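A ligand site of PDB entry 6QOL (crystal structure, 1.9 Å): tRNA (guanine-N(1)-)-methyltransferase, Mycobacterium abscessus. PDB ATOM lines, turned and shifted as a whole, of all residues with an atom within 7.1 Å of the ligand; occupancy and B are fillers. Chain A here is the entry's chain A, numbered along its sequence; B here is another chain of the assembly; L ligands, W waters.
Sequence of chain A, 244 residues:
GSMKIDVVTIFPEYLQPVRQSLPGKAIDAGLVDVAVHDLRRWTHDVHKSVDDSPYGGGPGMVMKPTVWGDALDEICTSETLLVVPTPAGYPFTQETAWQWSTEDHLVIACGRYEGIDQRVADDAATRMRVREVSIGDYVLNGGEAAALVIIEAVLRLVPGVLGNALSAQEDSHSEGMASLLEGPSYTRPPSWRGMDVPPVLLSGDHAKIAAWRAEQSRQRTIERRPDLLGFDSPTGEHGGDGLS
N of Leu 140 is in hydrogen-bond range of N2 of the ligand, 3.1 Å away.
A nitrogen (N1) of the ligand sits at hydrogen-bond distance from the backbone carbonyl oxygen (O) of Gly 111, 3.0 Å away.
A nitrogen (N1) of the ligand sits at hydrogen-bond distance from the backbone carbonyl oxygen (O) of Pro 85 (2.9 Å).
The side-chain hydroxyl of Tyr 138 is in hydrogen-bond range of the backbone carbonyl oxygen of Ile 135.
The backbone carbonyl oxygen of Thr 86 sits close to the backbone NH of Ser 134 (3.3 Å).
O of Gly 111 sits at hydrogen-bond distance from N of Gly 143, at 2.9 Å.
O of Gly 136 lies within hydrogen-bond range of OG of Ser 134 (2.8 Å).
The side-chain hydroxyl (OG1) of Thr 86 lies close to the backbone NH (N) of Ala 88, 3.3 Å away.
The backbone NH (N) of Thr 86 sits at hydrogen-bond distance from the backbone carbonyl oxygen (O) of Val 133, at 2.9 Å.
N of Tyr 113 is in hydrogen-bond range of O of Asn 141, at 3.0 Å.
N1 of the ligand lies close to N of Gly 143 (3.3 Å).
N of Thr 86 touches C8 of the ligand, at 3.3 Å.
Pro 87 touches the ligand.
CA of Tyr 113 touches C3 of the ligand, 3.7 Å away.
Gly 136 touches the ligand.
Tyr 138 touches the ligand (O to C6, 3.1 Å).
Val 139 touches the ligand.
C of Gly 142 touches C3 of the ligand (3.5 Å).
Along chain A the residues within 4 Å of the ligand span positions 85 to 143.
The nearest printed residue that does not touch the ligand is Arg 112 (4.1 Å).
Water W3 lies within hydrogen-bond range of a nitrogen (N3) of the ligand (2.8 Å), the backbone NH of Ile 135 (3.0 Å) and the backbone carbonyl oxygen of Val 133 (3.0 Å).
Water W1 lies within hydrogen-bond range of the backbone carbonyl oxygen of Arg 112 (2.9 Å), the backbone carbonyl oxygen of Tyr 113 (3.2 Å), a nitrogen (N1) of the ligand (3.3 Å) and the side-chain hydroxyl of Thr 86 (3.4 Å).
Water W2 lies within hydrogen-bond range of the backbone carbonyl oxygen (O) of Ala 109 (2.6 Å), the backbone carbonyl oxygen (O) of Pro 85 (2.7 Å), the backbone NH (N) of Gly 111 (2.8 Å) and a nitrogen (N1) of the ligand (3.5 Å).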
ATOM      1  N   VAL A  84      28.918  25.777  14.266  1.00  0.00           N
ATOM      2  CA  VAL A  84      28.538  24.575  15.001  1.00  0.00           C
ATOM      3  C   VAL A  84      28.641  24.848  16.502  1.00  0.00           C
ATOM      4  O   VAL A  84      29.743  24.838  17.079  1.00  0.00           O
ATOM      5  CB  VAL A  84      29.444  23.387  14.649  1.00  0.00           C
ATOM      6  CG1 VAL A  84      28.930  22.108  15.335  1.00  0.00           C
ATOM      7  CG2 VAL A  84      29.552  23.216  13.141  1.00  0.00           C
ATOM      8  N   PRO A  85      27.503  25.129  17.139  1.00  0.00           N
ATOM      9  CA  PRO A  85      27.576  25.350  18.592  1.00  0.00           C
ATOM     10  C   PRO A  85      27.939  24.050  19.298  1.00  0.00           C
ATOM     11  O   PRO A  85      27.352  23.005  19.040  1.00  0.00           O
ATOM     12  CB  PRO A  85      26.169  25.817  18.963  1.00  0.00           C
ATOM     13  CG  PRO A  85      25.577  26.346  17.650  1.00  0.00           C
ATOM     14  CD  PRO A  85      26.192  25.496  16.574  1.00  0.00           C
ATOM     15  N   THR A  86      28.791  23.988  20.277  1.00  0.00           N
ATOM     16  CA  THR A  86      29.424  22.863  20.955  1.00  0.00           C
ATOM     17  C   THR A  86      30.205  23.385  22.134  1.00  0.00           C
ATOM     18  O   THR A  86      30.783  24.474  22.065  1.00  0.00           O
ATOM     19  CB  THR A  86      30.359  22.048  20.025  1.00  0.00           C
ATOM     20  OG1 THR A  86      30.763  20.853  20.706  1.00  0.00           O
ATOM     21  CG2 THR A  86      31.594  22.818  19.667  1.00  0.00           C
ATOM     22  N   PRO A  87      29.897  22.487  23.207  1.00  0.00           N
ATOM     23  CA  PRO A  87      30.578  22.743  24.477  1.00  0.00           C
ATOM     24  C   PRO A  87      32.085  22.625  24.308  1.00  0.00           C
ATOM     25  O   PRO A  87      32.824  23.172  25.123  1.00  0.00           O
ATOM     26  CB  PRO A  87      30.034  21.643  25.398  1.00  0.00           C
ATOM     27  CG  PRO A  87      29.602  20.538  24.441  1.00  0.00           C
ATOM     28  CD  PRO A  87      29.059  21.268  23.259  1.00  0.00           C
ATOM     29  N   ALA A  88      32.548  21.940  23.260  1.00  0.00           N
ATOM     30  CA  ALA A  88      33.979  21.819  23.022  1.00  0.00           C
ATOM     31  C   ALA A  88      34.520  22.887  22.069  1.00  0.00           C
ATOM     32  O   ALA A  88      35.627  22.745  21.543  1.00  0.00           O
ATOM     33  CB  ALA A  88      34.314  20.415  22.477  1.00  0.00           C
ATOM     34  N   GLY A  89      33.738  23.935  21.838  1.00  0.00           N
ATOM     35  CA  GLY A  89      34.132  24.961  20.897  1.00  0.00           C
ATOM     36  C   GLY A  89      35.072  26.038  21.425  1.00  0.00           C
ATOM     37  O   GLY A  89      35.318  26.123  22.609  1.00  0.00           O
ATOM     38  N   ALA A 109      24.460  24.701  12.577  1.00  0.00           N
ATOM     39  CA  ALA A 109      24.151  23.289  12.698  1.00  0.00           C
ATOM     40  C   ALA A 109      23.968  22.891  14.148  1.00  0.00           C
ATOM     41  O   ALA A 109      24.940  22.800  14.898  1.00  0.00           O
ATOM     42  CB  ALA A 109      25.271  22.469  12.059  1.00  0.00           C
ATOM     43  N   CYS A 110      22.722  22.639  14.553  1.00  0.00           N
ATOM     44  CA  CYS A 110      22.410  22.354  15.947  1.00  0.00           C
ATOM     45  C   CYS A 110      22.408  20.864  16.228  1.00  0.00           C
ATOM     46  O   CYS A 110      21.581  20.145  15.683  1.00  0.00           O
ATOM     47  CB  CYS A 110      21.043  22.930  16.340  1.00  0.00           C
ATOM     48  SG  CYS A 110      20.913  24.727  16.080  1.00  0.00           S
ATOM     49  N   GLY A 111      23.300  20.416  17.107  1.00  0.00           N
ATOM     50  CA  GLY A 111      23.369  19.021  17.494  1.00  0.00           C
ATOM     51  C   GLY A 111      23.193  18.856  18.989  1.00  0.00           C
ATOM     52  O   GLY A 111      23.205  19.827  19.745  1.00  0.00           O
ATOM     53  N   ARG A 112      23.044  17.611  19.427  1.00  0.00           N
ATOM     54  CA  ARG A 112      22.959  17.313  20.852  1.00  0.00           C
ATOM     55  C   ARG A 112      24.319  17.515  21.533  1.00  0.00           C
ATOM     56  O   ARG A 112      25.343  17.622  20.854  1.00  0.00           O
ATOM     57  CB  ARG A 112      22.469  15.880  21.051  1.00  0.00           C
ATOM     58  CG  ARG A 112      23.286  14.843  20.284  1.00  0.00           C
ATOM     59  CD  ARG A 112      22.667  13.445  20.388  1.00  0.00           C
ATOM     60  NE  ARG A 112      22.711  12.936  21.756  1.00  0.00           N
ATOM     61  CZ  ARG A 112      21.833  12.071  22.270  1.00  0.00           C
ATOM     62  NH1 ARG A 112      20.830  11.620  21.525  1.00  0.00           N
ATOM     63  NH2 ARG A 112      21.944  11.660  23.522  1.00  0.00           N
ATOM     64  N   TYR A 113      24.322  17.556  22.867  1.00  0.00           N
ATOM     65  CA  TYR A 113      25.557  17.786  23.629  1.00  0.00           C
ATOM     66  C   TYR A 113      26.710  16.891  23.167  1.00  0.00           C
ATOM     67  O   TYR A 113      27.828  17.371  22.951  1.00  0.00           O
ATOM     68  CB  TYR A 113      25.316  17.557  25.132  1.00  0.00           C
ATOM     69  CG  TYR A 113      26.583  17.753  25.928  1.00  0.00           C
ATOM     70  CD1 TYR A 113      26.953  19.025  26.357  1.00  0.00           C
ATOM     71  CD2 TYR A 113      27.417  16.687  26.236  1.00  0.00           C
ATOM     72  CE1 TYR A 113      28.120  19.218  27.083  1.00  0.00           C
ATOM     73  CE2 TYR A 113      28.596  16.881  26.955  1.00  0.00           C
ATOM     74  CZ  TYR A 113      28.938  18.151  27.376  1.00  0.00           C
ATOM     75  OH  TYR A 113      30.093  18.383  28.091  1.00  0.00           O
ATOM     76  N   GLU A 114      26.411  15.614  22.997  1.00  0.00           N
ATOM     77  CA  GLU A 114      27.411  14.615  22.610  1.00  0.00           C
ATOM     78  C   GLU A 114      28.066  14.905  21.269  1.00  0.00           C
ATOM     79  O   GLU A 114      29.196  14.498  21.023  1.00  0.00           O
ATOM     80  CB  GLU A 114      26.783  13.221  22.589  1.00  0.00           C
ATOM     81  CG  GLU A 114      26.321  12.700  23.957  1.00  0.00           C
ATOM     82  CD  GLU A 114      24.974  13.251  24.408  1.00  0.00           C
ATOM     83  OE1 GLU A 114      24.367  14.067  23.676  1.00  0.00           O
ATOM     84  OE2 GLU A 114      24.513  12.850  25.495  1.00  0.00           O
ATOM     85  N   GLY A 115      27.336  15.594  20.397  1.00  0.00           N
ATOM     86  CA  GLY A 115      27.929  16.152  19.200  1.00  0.00           C
ATOM     87  C   GLY A 115      27.622  15.421  17.913  1.00  0.00           C
ATOM     88  O   GLY A 115      26.870  14.450  17.875  1.00  0.00           O
ATOM     89  N   VAL A 133      31.929  26.664  18.208  1.00  0.00           N
ATOM     90  CA  VAL A 133      31.975  27.665  19.287  1.00  0.00           C
ATOM     91  C   VAL A 133      31.108  27.281  20.482  1.00  0.00           C
ATOM     92  O   VAL A 133      30.076  26.634  20.327  1.00  0.00           O
ATOM     93  CB  VAL A 133      31.525  29.068  18.790  1.00  0.00           C
ATOM     94  CG1 VAL A 133      32.450  29.582  17.705  1.00  0.00           C
ATOM     95  CG2 VAL A 133      30.104  29.022  18.262  1.00  0.00           C
ATOM     96  N   SER A 134      31.565  27.678  21.681  1.00  0.00           N
ATOM     97  CA  SER A 134      30.783  27.502  22.907  1.00  0.00           C
ATOM     98  C   SER A 134      30.313  28.854  23.441  1.00  0.00           C
ATOM     99  O   SER A 134      31.123  29.781  23.621  1.00  0.00           O
ATOM    100  CB  SER A 134      31.610  26.777  23.970  1.00  0.00           C
ATOM    101  OG  SER A 134      31.086  26.946  25.283  1.00  0.00           O
ATOM    102  N   ILE A 135      29.012  28.974  23.725  1.00  0.00           N
ATOM    103  CA  ILE A 135      28.488  30.210  24.317  1.00  0.00           C
ATOM    104  C   ILE A 135      28.735  30.294  25.827  1.00  0.00           C
ATOM    105  O   ILE A 135      28.490  31.343  26.424  1.00  0.00           O
ATOM    106  CB  ILE A 135      26.958  30.393  24.075  1.00  0.00           C
ATOM    107  CG1 ILE A 135      26.147  29.222  24.678  1.00  0.00           C
ATOM    108  CG2 ILE A 135      26.672  30.571  22.596  1.00  0.00           C
ATOM    109  CD1 ILE A 135      24.698  29.573  24.974  1.00  0.00           C
ATOM    110  N   GLY A 136      29.240  29.216  26.429  1.00  0.00           N
ATOM    111  CA  GLY A 136      29.542  29.225  27.849  1.00  0.00           C
ATOM    112  C   GLY A 136      29.893  27.855  28.413  1.00  0.00           C
ATOM    113  O   GLY A 136      29.748  26.830  27.726  1.00  0.00           O
ATOM    114  N   ASP A 137      30.326  27.833  29.671  1.00  0.00           N
ATOM    115  CA  ASP A 137      30.848  26.591  30.236  1.00  0.00           C
ATOM    116  C   ASP A 137      29.838  25.846  31.111  1.00  0.00           C
ATOM    117  O   ASP A 137      30.208  25.088  31.998  1.00  0.00           O
ATOM    118  CB  ASP A 137      32.132  26.871  31.014  1.00  0.00           C
ATOM    119  CG  ASP A 137      33.337  26.955  30.087  1.00  0.00           C
ATOM    120  OD1 ASP A 137      33.262  26.423  28.942  1.00  0.00           O
ATOM    121  OD2 ASP A 137      34.359  27.558  30.472  1.00  0.00           O
ATOM    122  N   TYR A 138      28.570  26.069  30.828  1.00  0.00           N
ATOM    123  CA  TYR A 138      27.493  25.290  31.410  1.00  0.00           C
ATOM    124  C   TYR A 138      27.104  24.283  30.337  1.00  0.00           C
ATOM    125  O   TYR A 138      27.489  24.424  29.187  1.00  0.00           O
ATOM    126  CB  TYR A 138      26.322  26.177  31.802  1.00  0.00           C
ATOM    127  CG  TYR A 138      26.212  27.356  30.877  1.00  0.00           C
ATOM    128  CD1 TYR A 138      25.670  27.218  29.603  1.00  0.00           C
ATOM    129  CD2 TYR A 138      26.702  28.606  31.250  1.00  0.00           C
ATOM    130  CE1 TYR A 138      25.597  28.308  28.733  1.00  0.00           C
ATOM    131  CE2 TYR A 138      26.637  29.690  30.378  1.00  0.00           C
ATOM    132  CZ  TYR A 138      26.090  29.536  29.136  1.00  0.00           C
ATOM    133  OH  TYR A 138      26.037  30.614  28.284  1.00  0.00           O
ATOM    134  N   VAL A 139      26.335  23.275  30.718  1.00  0.00           N
ATOM    135  CA  VAL A 139      25.963  22.213  29.798  1.00  0.00           C
ATOM    136  C   VAL A 139      24.488  22.277  29.438  1.00  0.00           C
ATOM    137  O   VAL A 139      23.635  22.259  30.319  1.00  0.00           O
ATOM    138  CB  VAL A 139      26.248  20.807  30.395  1.00  0.00           C
ATOM    139  CG1 VAL A 139      25.704  19.745  29.471  1.00  0.00           C
ATOM    140  CG2 VAL A 139      27.738  20.623  30.620  1.00  0.00           C
ATOM    141  N   LEU A 140      24.203  22.365  28.146  1.00  0.00           N
ATOM    142  CA  LEU A 140      22.835  22.306  27.622  1.00  0.00           C
ATOM    143  C   LEU A 140      22.632  20.926  27.042  1.00  0.00           C
ATOM    144  O   LEU A 140      23.612  20.234  26.753  1.00  0.00           O
ATOM    145  CB  LEU A 140      22.616  23.349  26.532  1.00  0.00           C
ATOM    146  CG  LEU A 140      23.011  24.793  26.884  1.00  0.00           C
ATOM    147  CD1 LEU A 140      22.824  25.696  25.683  1.00  0.00           C
ATOM    148  CD2 LEU A 140      22.207  25.292  28.065  1.00  0.00           C
ATOM    149  N   ASN A 141      21.393  20.522  26.804  1.00  0.00           N
ATOM    150  CA  ASN A 141      21.134  19.234  26.179  1.00  0.00           C
ATOM    151  C   ASN A 141      21.339  19.262  24.677  1.00  0.00           C
ATOM    152  O   ASN A 141      21.699  18.260  24.068  1.00  0.00           O
ATOM    153  CB  ASN A 141      19.724  18.751  26.469  1.00  0.00           C
ATOM    154  CG  ASN A 141      19.719  17.373  27.045  1.00  0.00           C
ATOM    155  OD1 ASN A 141      20.441  17.085  28.009  1.00  0.00           O
ATOM    156  ND2 ASN A 141      18.931  16.486  26.455  1.00  0.00           N
ATOM    157  N   GLY A 142      21.108  20.423  24.071  1.00  0.00           N
ATOM    158  CA  GLY A 142      21.206  20.562  22.633  1.00  0.00           C
ATOM    159  C   GLY A 142      21.638  21.970  22.283  1.00  0.00           C
ATOM    160  O   GLY A 142      21.604  22.848  23.120  1.00  0.00           O
ATOM    161  N   GLY A 143      22.066  22.163  21.047  1.00  0.00           N
ATOM    162  CA  GLY A 143      22.582  23.463  20.620  1.00  0.00           C
ATOM    163  C   GLY A 143      21.550  24.517  20.266  1.00  0.00           C
ATOM    164  O   GLY A 143      21.909  25.646  19.930  1.00  0.00           O
ATOM    165  N   GLU A 144      20.254  24.171  20.358  1.00  0.00           N
ATOM    166  CA  GLU A 144      19.215  25.119  19.955  1.00  0.00           C
ATOM    167  C   GLU A 144      19.246  26.434  20.755  1.00  0.00           C
ATOM    168  O   GLU A 144      19.178  27.522  20.174  1.00  0.00           O
ATOM    169  CB  GLU A 144      17.829  24.477  20.099  1.00  0.00           C
ATOM    170  CG  GLU A 144      17.495  23.495  18.968  1.00  0.00           C
ATOM    171  CD  GLU A 144      18.256  22.180  19.069  1.00  0.00           C
ATOM    172  OE1 GLU A 144      18.706  21.806  20.177  1.00  0.00           O
ATOM    173  OE2 GLU A 144      18.409  21.526  18.009  1.00  0.00           O
ATOM    174  N   ALA A 146      21.780  27.699  22.284  1.00  0.00           N
ATOM    175  CA  ALA A 146      23.004  28.380  21.860  1.00  0.00           C
ATOM    176  C   ALA A 146      22.841  29.087  20.516  1.00  0.00           C
ATOM    177  O   ALA A 146      23.369  30.195  20.310  1.00  0.00           O
ATOM    178  CB  ALA A 146      24.169  27.390  21.792  1.00  0.00           C
ATOM    179  N   ALA A 147      22.116  28.448  19.591  1.00  0.00           N
ATOM    180  CA  ALA A 147      21.821  29.068  18.305  1.00  0.00           C
ATOM    181  C   ALA A 147      21.033  30.354  18.484  1.00  0.00           C
ATOM    182  O   ALA A 147      21.266  31.345  17.781  1.00  0.00           O
ATOM    183  CB  ALA A 147      21.032  28.096  17.375  1.00  0.00           C
ATOM    184  N   GLU B 152      17.335  25.619  30.582  1.00  0.00           N
ATOM    185  CA  GLU B 152      17.784  24.354  30.023  1.00  0.00           C
ATOM    186  C   GLU B 152      18.940  23.761  30.817  1.00  0.00           C
ATOM    187  O   GLU B 152      18.979  22.550  31.039  1.00  0.00           O
ATOM    188  CB  GLU B 152      18.192  24.525  28.572  1.00  0.00           C
ATOM    189  CG  GLU B 152      18.708  23.228  27.961  1.00  0.00           C
ATOM    190  CD  GLU B 152      18.160  23.002  26.584  1.00  0.00           C
ATOM    191  OE1 GLU B 152      17.360  23.849  26.125  1.00  0.00           O
ATOM    192  OE2 GLU B 152      18.529  21.978  25.968  1.00  0.00           O
HETATM  193  C1  LIG L   1      26.405  23.742  23.607  1.00  0.00           C
HETATM  194  N1  LIG L   1      25.315  21.715  20.640  1.00  0.00           N
HETATM  195  C2  LIG L   1      25.516  22.144  21.977  1.00  0.00           C
HETATM  196  C3  LIG L   1      25.013  21.362  23.023  1.00  0.00           C
HETATM  197  C4  LIG L   1      25.214  21.763  24.336  1.00  0.00           C
HETATM  198  C5  LIG L   1      25.919  22.974  24.628  1.00  0.00           C
HETATM  199  N2  LIG L   1      26.104  23.348  25.947  1.00  0.00           N
HETATM  200  C6  LIG L   1      26.772  24.491  26.223  1.00  0.00           C
HETATM  201  C7  LIG L   1      27.267  25.295  25.184  1.00  0.00           C
HETATM  202  N3  LIG L   1      27.081  24.912  23.892  1.00  0.00           N
HETATM  203  C8  LIG L   1      26.200  23.330  22.253  1.00  0.00           C
HETATM  204  O   HOH W   1      27.666  19.363  20.451  1.00  0.00           O
HETATM  205  O   HOH W   2      25.690  21.915  17.200  1.00  0.00           O
HETATM  206  O   HOH W   3      27.616  26.969  22.007  1.00  0.00           O
